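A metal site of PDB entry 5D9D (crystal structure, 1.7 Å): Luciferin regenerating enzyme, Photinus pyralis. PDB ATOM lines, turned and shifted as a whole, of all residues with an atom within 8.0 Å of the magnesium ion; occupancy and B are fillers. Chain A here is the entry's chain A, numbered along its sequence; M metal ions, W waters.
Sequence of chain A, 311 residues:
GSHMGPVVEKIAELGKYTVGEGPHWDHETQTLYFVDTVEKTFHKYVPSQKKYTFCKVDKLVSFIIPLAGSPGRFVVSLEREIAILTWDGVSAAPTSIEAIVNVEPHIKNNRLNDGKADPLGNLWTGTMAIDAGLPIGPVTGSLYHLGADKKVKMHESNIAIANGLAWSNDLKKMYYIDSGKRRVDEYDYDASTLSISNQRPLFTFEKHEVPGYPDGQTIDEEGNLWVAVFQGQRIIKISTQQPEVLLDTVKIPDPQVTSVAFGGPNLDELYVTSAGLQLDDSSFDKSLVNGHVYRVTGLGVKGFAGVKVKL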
ATOM      1  N   VAL A  19      -3.939 -24.878  27.285  1.00  0.00           N
ATOM      2  CA  VAL A  19      -2.673 -25.128  26.592  1.00  0.00           C
ATOM      3  C   VAL A  19      -1.588 -25.390  27.692  1.00  0.00           C
ATOM      4  O   VAL A  19      -0.836 -24.474  28.042  1.00  0.00           O
ATOM      5  CB  VAL A  19      -2.232 -23.980  25.647  1.00  0.00           C
ATOM      6  CG1 VAL A  19      -0.890 -24.410  24.861  1.00  0.00           C
ATOM      7  CG2 VAL A  19      -3.302 -23.669  24.531  1.00  0.00           C
ATOM      8  N   GLY A  20      -1.503 -26.652  28.135  1.00  0.00           N
ATOM      9  CA  GLY A  20      -0.402 -27.032  29.070  1.00  0.00           C
ATOM     10  C   GLY A  20       0.903 -26.931  28.310  1.00  0.00           C
ATOM     11  O   GLY A  20       0.952 -27.276  27.133  1.00  0.00           O
ATOM     12  N   GLU A  21       1.953 -26.375  28.932  1.00  0.00           N
ATOM     13  CA  GLU A  21       3.219 -26.095  28.208  1.00  0.00           C
ATOM     14  C   GLU A  21       4.350 -25.904  29.190  1.00  0.00           C
ATOM     15  O   GLU A  21       4.117 -25.879  30.373  1.00  0.00           O
ATOM     16  CB  GLU A  21       3.080 -24.770  27.387  1.00  0.00           C
ATOM     17  CG  GLU A  21       2.815 -25.065  25.897  1.00  0.00           C
ATOM     18  CD  GLU A  21       4.089 -25.451  25.158  1.00  0.00           C
ATOM     19  OE1 GLU A  21       4.017 -25.450  23.890  1.00  0.00           O
ATOM     20  OE2 GLU A  21       5.110 -25.738  25.819  1.00  0.00           O
ATOM     21  N   GLY A  22       5.566 -25.742  28.681  1.00  0.00           N
ATOM     22  CA  GLY A  22       6.700 -25.318  29.514  1.00  0.00           C
ATOM     23  C   GLY A  22       7.049 -26.215  30.702  1.00  0.00           C
ATOM     24  O   GLY A  22       7.409 -25.680  31.727  1.00  0.00           O
ATOM     25  N   PRO A  23       7.011 -27.551  30.565  1.00  0.00           N
ATOM     26  CA  PRO A  23       7.362 -28.366  31.737  1.00  0.00           C
ATOM     27  C   PRO A  23       8.838 -28.211  32.111  1.00  0.00           C
ATOM     28  O   PRO A  23       9.735 -28.103  31.243  1.00  0.00           O
ATOM     29  CB  PRO A  23       7.099 -29.814  31.286  1.00  0.00           C
ATOM     30  CG  PRO A  23       7.336 -29.763  29.740  1.00  0.00           C
ATOM     31  CD  PRO A  23       6.706 -28.382  29.366  1.00  0.00           C
ATOM     32  N   THR A  37      -0.682 -21.568  28.998  1.00  0.00           N
ATOM     33  CA  THR A  37      -0.485 -20.237  28.459  1.00  0.00           C
ATOM     34  C   THR A  37      -1.766 -19.385  28.526  1.00  0.00           C
ATOM     35  O   THR A  37      -1.761 -18.233  29.107  1.00  0.00           O
ATOM     36  CB  THR A  37       0.019 -20.363  27.066  1.00  0.00           C
ATOM     37  OG1 THR A  37      -0.943 -21.071  26.260  1.00  0.00           O
ATOM     38  CG2 THR A  37       1.291 -21.185  27.048  1.00  0.00           C
ATOM     39  N   SER A  62       4.327 -18.199  29.410  1.00  0.00           N
ATOM     40  CA  SER A  62       4.742 -19.300  28.546  1.00  0.00           C
ATOM     41  C   SER A  62       5.894 -20.156  29.100  1.00  0.00           C
ATOM     42  O   SER A  62       6.178 -21.216  28.579  1.00  0.00           O
ATOM     43  CB  SER A  62       5.121 -18.746  27.158  1.00  0.00           C
ATOM     44  OG  SER A  62       6.287 -17.929  27.294  1.00  0.00           O
ATOM     45  N   ARG A 111       3.888 -11.874  21.758  1.00  0.00           N
ATOM     46  CA  ARG A 111       4.099 -12.409  23.095  1.00  0.00           C
ATOM     47  C   ARG A 111       5.300 -13.317  23.092  1.00  0.00           C
ATOM     48  O   ARG A 111       5.725 -13.813  22.034  1.00  0.00           O
ATOM     49  CB  ARG A 111       2.878 -13.206  23.573  1.00  0.00           C
ATOM     50  CG  ARG A 111       2.702 -14.570  22.903  1.00  0.00           C
ATOM     51  CD  ARG A 111       1.547 -15.370  23.560  1.00  0.00           C
ATOM     52  NE  ARG A 111       1.131 -16.549  22.815  1.00  0.00           N
ATOM     53  CZ  ARG A 111       1.653 -17.772  22.969  1.00  0.00           C
ATOM     54  NH1 ARG A 111       1.204 -18.789  22.233  1.00  0.00           N
ATOM     55  NH2 ARG A 111       2.624 -17.977  23.832  1.00  0.00           N
ATOM     56  N   ASN A 113       6.966 -16.973  23.714  1.00  0.00           N
ATOM     57  CA  ASN A 113       6.476 -18.365  23.745  1.00  0.00           C
ATOM     58  C   ASN A 113       7.545 -19.202  24.388  1.00  0.00           C
ATOM     59  O   ASN A 113       7.921 -18.900  25.548  1.00  0.00           O
ATOM     60  CB  ASN A 113       6.068 -18.840  22.349  1.00  0.00           C
ATOM     61  CG  ASN A 113       5.158 -20.075  22.423  1.00  0.00           C
ATOM     62  OD1 ASN A 113       4.403 -20.258  23.388  1.00  0.00           O
ATOM     63  ND2 ASN A 113       5.296 -20.956  21.462  1.00  0.00           N
ATOM     64  N   ASP A 114       8.073 -20.229  23.730  1.00  0.00           N
ATOM     65  CA  ASP A 114       8.828 -21.198  24.519  1.00  0.00           C
ATOM     66  C   ASP A 114      10.172 -20.593  24.997  1.00  0.00           C
ATOM     67  O   ASP A 114      10.729 -19.750  24.305  1.00  0.00           O
ATOM     68  CB  ASP A 114       9.082 -22.445  23.699  1.00  0.00           C
ATOM     69  CG  ASP A 114       9.273 -23.707  24.590  1.00  0.00           C
ATOM     70  OD1 ASP A 114       9.240 -23.595  25.860  1.00  0.00           O
ATOM     71  OD2 ASP A 114       9.472 -24.798  24.026  1.00  0.00           O
ATOM     72  N   GLY A 115      10.646 -21.013  26.167  1.00  0.00           N
ATOM     73  CA  GLY A 115      11.896 -20.478  26.674  1.00  0.00           C
ATOM     74  C   GLY A 115      12.553 -21.573  27.507  1.00  0.00           C
ATOM     75  O   GLY A 115      11.865 -22.419  28.111  1.00  0.00           O
ATOM     76  N   MET A 128       6.349 -14.393  19.136  1.00  0.00           N
ATOM     77  CA  MET A 128       5.445 -14.694  18.042  1.00  0.00           C
ATOM     78  C   MET A 128       4.236 -13.793  18.130  1.00  0.00           C
ATOM     79  O   MET A 128       3.984 -13.181  19.174  1.00  0.00           O
ATOM     80  CB  MET A 128       5.016 -16.159  18.141  1.00  0.00           C
ATOM     81  CG  MET A 128       4.327 -16.437  19.485  1.00  0.00           C
ATOM     82  SD  MET A 128       3.763 -18.183  19.596  1.00  0.00           S
ATOM     83  CE  MET A 128       2.227 -18.095  18.690  1.00  0.00           C
ATOM     84  N   ILE A 161       6.253 -19.376  14.748  1.00  0.00           N
ATOM     85  CA  ILE A 161       5.822 -19.898  16.071  1.00  0.00           C
ATOM     86  C   ILE A 161       7.058 -20.366  16.841  1.00  0.00           C
ATOM     87  O   ILE A 161       7.551 -21.447  16.609  1.00  0.00           O
ATOM     88  CB  ILE A 161       4.777 -21.028  15.905  1.00  0.00           C
ATOM     89  CG1 ILE A 161       3.576 -20.441  15.096  1.00  0.00           C
ATOM     90  CG2 ILE A 161       4.284 -21.498  17.302  1.00  0.00           C
ATOM     91  CD1 ILE A 161       2.452 -21.429  14.776  1.00  0.00           C
ATOM     92  N   ALA A 162       7.559 -19.509  17.732  1.00  0.00           N
ATOM     93  CA  ALA A 162       8.823 -19.724  18.439  1.00  0.00           C
ATOM     94  C   ALA A 162       8.642 -20.869  19.410  1.00  0.00           C
ATOM     95  O   ALA A 162       7.862 -20.742  20.408  1.00  0.00           O
ATOM     96  CB  ALA A 162       9.222 -18.439  19.180  1.00  0.00           C
ATOM     97  N   ASN A 163       9.317 -21.993  19.162  1.00  0.00           N
ATOM     98  CA  ASN A 163       9.029 -23.156  20.018  1.00  0.00           C
ATOM     99  C   ASN A 163      10.277 -23.837  20.512  1.00  0.00           C
ATOM    100  O   ASN A 163      11.164 -23.146  21.042  1.00  0.00           O
ATOM    101  CB  ASN A 163       8.044 -24.109  19.290  1.00  0.00           C
ATOM    102  CG  ASN A 163       6.709 -24.064  19.938  1.00  0.00           C
ATOM    103  OD1 ASN A 163       6.661 -23.977  21.208  1.00  0.00           O
ATOM    104  ND2 ASN A 163       5.621 -24.066  19.164  1.00  0.00           N
ATOM    105  N   GLY A 164      10.298 -25.172  20.546  1.00  0.00           N
ATOM    106  CA  GLY A 164      11.263 -25.882  21.402  1.00  0.00           C
ATOM    107  C   GLY A 164      12.752 -25.640  21.166  1.00  0.00           C
ATOM    108  O   GLY A 164      13.171 -25.378  20.042  1.00  0.00           O
ATOM    109  N   ILE A 177      13.078 -25.096  17.067  1.00  0.00           N
ATOM    110  CA  ILE A 177      11.869 -25.330  16.290  1.00  0.00           C
ATOM    111  C   ILE A 177      11.046 -24.073  16.064  1.00  0.00           C
ATOM    112  O   ILE A 177      10.649 -23.431  17.020  1.00  0.00           O
ATOM    113  CB  ILE A 177      10.987 -26.382  17.031  1.00  0.00           C
ATOM    114  CG1 ILE A 177      11.706 -27.766  17.018  1.00  0.00           C
ATOM    115  CG2 ILE A 177       9.566 -26.492  16.402  1.00  0.00           C
ATOM    116  CD1 ILE A 177      11.169 -28.770  18.042  1.00  0.00           C
ATOM    117  N   SER A 179       7.560 -23.810  14.678  1.00  0.00           N
ATOM    118  CA  SER A 179       6.536 -24.814  14.339  1.00  0.00           C
ATOM    119  C   SER A 179       5.993 -24.627  12.906  1.00  0.00           C
ATOM    120  O   SER A 179       5.592 -25.589  12.268  1.00  0.00           O
ATOM    121  CB  SER A 179       5.345 -24.759  15.287  1.00  0.00           C
ATOM    122  OG  SER A 179       5.842 -25.121  16.576  1.00  0.00           O
ATOM    123  N   PRO A 214       5.990 -29.835  14.846  1.00  0.00           N
ATOM    124  CA  PRO A 214       6.879 -29.937  16.015  1.00  0.00           C
ATOM    125  C   PRO A 214       6.598 -28.777  16.993  1.00  0.00           C
ATOM    126  O   PRO A 214       6.252 -27.610  16.589  1.00  0.00           O
ATOM    127  CB  PRO A 214       8.310 -29.841  15.386  1.00  0.00           C
ATOM    128  CG  PRO A 214       8.079 -28.985  14.152  1.00  0.00           C
ATOM    129  CD  PRO A 214       6.695 -29.388  13.624  1.00  0.00           C
ATOM    130  N   ASP A 215       6.686 -29.070  18.298  1.00  0.00           N
ATOM    131  CA  ASP A 215       6.357 -27.986  19.277  1.00  0.00           C
ATOM    132  C   ASP A 215       7.514 -27.928  20.256  1.00  0.00           C
ATOM    133  O   ASP A 215       8.579 -27.399  19.882  1.00  0.00           O
ATOM    134  CB  ASP A 215       5.001 -28.282  19.929  1.00  0.00           C
ATOM    135  CG  ASP A 215       4.427 -27.094  20.715  1.00  0.00           C
ATOM    136  OD1 ASP A 215       5.207 -26.334  21.268  1.00  0.00           O
ATOM    137  OD2 ASP A 215       3.209 -27.071  20.850  1.00  0.00           O
ATOM    138  N   GLY A 216       7.395 -28.519  21.460  1.00  0.00           N
ATOM    139  CA  GLY A 216       8.529 -28.554  22.399  1.00  0.00           C
ATOM    140  C   GLY A 216       9.478 -29.708  22.137  1.00  0.00           C
ATOM    141  O   GLY A 216       9.128 -30.658  21.436  1.00  0.00           O
ATOM    142  N   GLN A 217      10.689 -29.645  22.678  1.00  0.00           N
ATOM    143  CA  GLN A 217      11.657 -30.751  22.506  1.00  0.00           C
ATOM    144  C   GLN A 217      12.613 -30.789  23.654  1.00  0.00           C
ATOM    145  O   GLN A 217      12.762 -29.807  24.434  1.00  0.00           O
ATOM    146  CB  GLN A 217      12.398 -30.600  21.195  1.00  0.00           C
ATOM    147  CG  GLN A 217      13.355 -29.406  21.173  1.00  0.00           C
ATOM    148  CD  GLN A 217      14.196 -29.376  19.874  1.00  0.00           C
ATOM    149  OE1 GLN A 217      14.412 -30.420  19.224  1.00  0.00           O
ATOM    150  NE2 GLN A 217      14.566 -28.175  19.436  1.00  0.00           N
ATOM    151  N   ALA A 228       7.806 -33.133  20.731  1.00  0.00           N
ATOM    152  CA  ALA A 228       6.345 -33.207  20.836  1.00  0.00           C
ATOM    153  C   ALA A 228       5.732 -32.844  19.531  1.00  0.00           C
ATOM    154  O   ALA A 228       6.106 -31.860  18.929  1.00  0.00           O
ATOM    155  CB  ALA A 228       5.868 -32.217  21.913  1.00  0.00           C
ATOM    156  N   PHE A 230       2.434 -31.603  17.920  1.00  0.00           N
ATOM    157  CA  PHE A 230       1.152 -30.974  18.071  1.00  0.00           C
ATOM    158  C   PHE A 230       0.255 -31.352  16.853  1.00  0.00           C
ATOM    159  O   PHE A 230       0.652 -31.100  15.700  1.00  0.00           O
ATOM    160  CB  PHE A 230       1.377 -29.426  18.121  1.00  0.00           C
ATOM    161  CG  PHE A 230       0.140 -28.655  18.524  1.00  0.00           C
ATOM    162  CD1 PHE A 230      -0.092 -28.405  19.855  1.00  0.00           C
ATOM    163  CD2 PHE A 230      -0.790 -28.217  17.563  1.00  0.00           C
ATOM    164  CE1 PHE A 230      -1.268 -27.672  20.232  1.00  0.00           C
ATOM    165  CE2 PHE A 230      -1.964 -27.521  17.933  1.00  0.00           C
ATOM    166  CZ  PHE A 230      -2.179 -27.258  19.272  1.00  0.00           C
ATOM    167  N   VAL A 257      -0.198 -32.692  21.475  1.00  0.00           N
ATOM    168  CA  VAL A 257       0.946 -32.804  22.410  1.00  0.00           C
ATOM    169  C   VAL A 257       1.774 -31.531  22.284  1.00  0.00           C
ATOM    170  O   VAL A 257       2.087 -31.131  21.174  1.00  0.00           O
ATOM    171  CB  VAL A 257       1.855 -34.031  22.007  1.00  0.00           C
ATOM    172  CG1 VAL A 257       2.944 -34.201  22.998  1.00  0.00           C
ATOM    173  CG2 VAL A 257       0.954 -35.295  22.018  1.00  0.00           C
ATOM    174  N   THR A 258       2.204 -30.945  23.400  1.00  0.00           N
ATOM    175  CA  THR A 258       2.880 -29.635  23.277  1.00  0.00           C
ATOM    176  C   THR A 258       4.337 -29.680  23.721  1.00  0.00           C
ATOM    177  O   THR A 258       5.164 -29.041  23.083  1.00  0.00           O
ATOM    178  CB  THR A 258       2.170 -28.526  24.147  1.00  0.00           C
ATOM    179  OG1 THR A 258       2.066 -29.017  25.497  1.00  0.00           O
ATOM    180  CG2 THR A 258       0.742 -28.230  23.583  1.00  0.00           C
ATOM    181  N   SER A 259       4.663 -30.410  24.776  1.00  0.00           N
ATOM    182  CA  SER A 259       6.087 -30.376  25.188  1.00  0.00           C
ATOM    183  C   SER A 259       6.445 -31.520  26.045  1.00  0.00           C
ATOM    184  O   SER A 259       5.590 -32.360  26.334  1.00  0.00           O
ATOM    185  CB  SER A 259       6.425 -29.031  25.884  1.00  0.00           C
ATOM    186  OG  SER A 259       7.845 -28.798  25.986  1.00  0.00           O
ATOM    187  N   THR A 273       3.199 -32.600  28.206  1.00  0.00           N
ATOM    188  CA  THR A 273       2.021 -31.740  28.345  1.00  0.00           C
ATOM    189  C   THR A 273       1.193 -31.773  27.047  1.00  0.00           C
ATOM    190  O   THR A 273       1.720 -32.110  25.972  1.00  0.00           O
ATOM    191  CB  THR A 273       2.407 -30.278  28.649  1.00  0.00           C
ATOM    192  OG1 THR A 273       3.397 -29.839  27.717  1.00  0.00           O
ATOM    193  CG2 THR A 273       3.025 -30.146  30.067  1.00  0.00           C
HETATM  194 MG    MG M   1       5.408 -24.833  22.614  1.00  0.00          MG
HETATM  195  O   HOH W   1       5.713 -23.102  23.906  1.00  0.00           O
HETATM  196  O   HOH W   2       3.745 -23.755  21.809  1.00  0.00           O
HETATM  197  O   HOH W   3       6.758 -25.792  23.685  1.00  0.00           O
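Water W1 lies within hydrogen-bond range of OD1 of Asn 113 and OE2 of Glu 21. Water W2 lies within hydrogen-bond range of ND2 of Asn 113 (3.2 Å), ND2 of Asn 163 (3.3 Å) and OD2 of Asp 215 (3.5 Å). Water W3 lies within hydrogen-bond range of OE2 of Glu 21 and OD2 of Asp 114.
The backbone carbonyl oxygen of Asp 215 is in hydrogen-bond range of the backbone NH of Gly 164, 2.9 Å away. N of Asp 215 sits at hydrogen-bond distance from O of Ala 228, 2.9 Å away. The side-chain amide oxygen of Asn 163 lies close to the side-chain amide nitrogen of Asn 113 (3.3 Å). The side-chain hydroxyl of Ser 179 sits at hydrogen-bond distance from the side-chain amide nitrogen of Asn 163 (2.8 Å). The backbone carbonyl oxygen (O) of Ile 177 is in hydrogen-bond range of the backbone NH (N) of Asn 163.
The magnesium ion is bound by water W3 (2.0 Å), OE1 of Glu 21 (2.0 Å), OD1 of Asp 215 (2.0 Å), OD1 of Asn 163 (2.1 Å), water W2 (2.1 Å) and water W1 (2.2 Å).
Three residues have an atom within 4 Å of the magnesium ion: Glu 21, Asn 163 and Asp 215.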
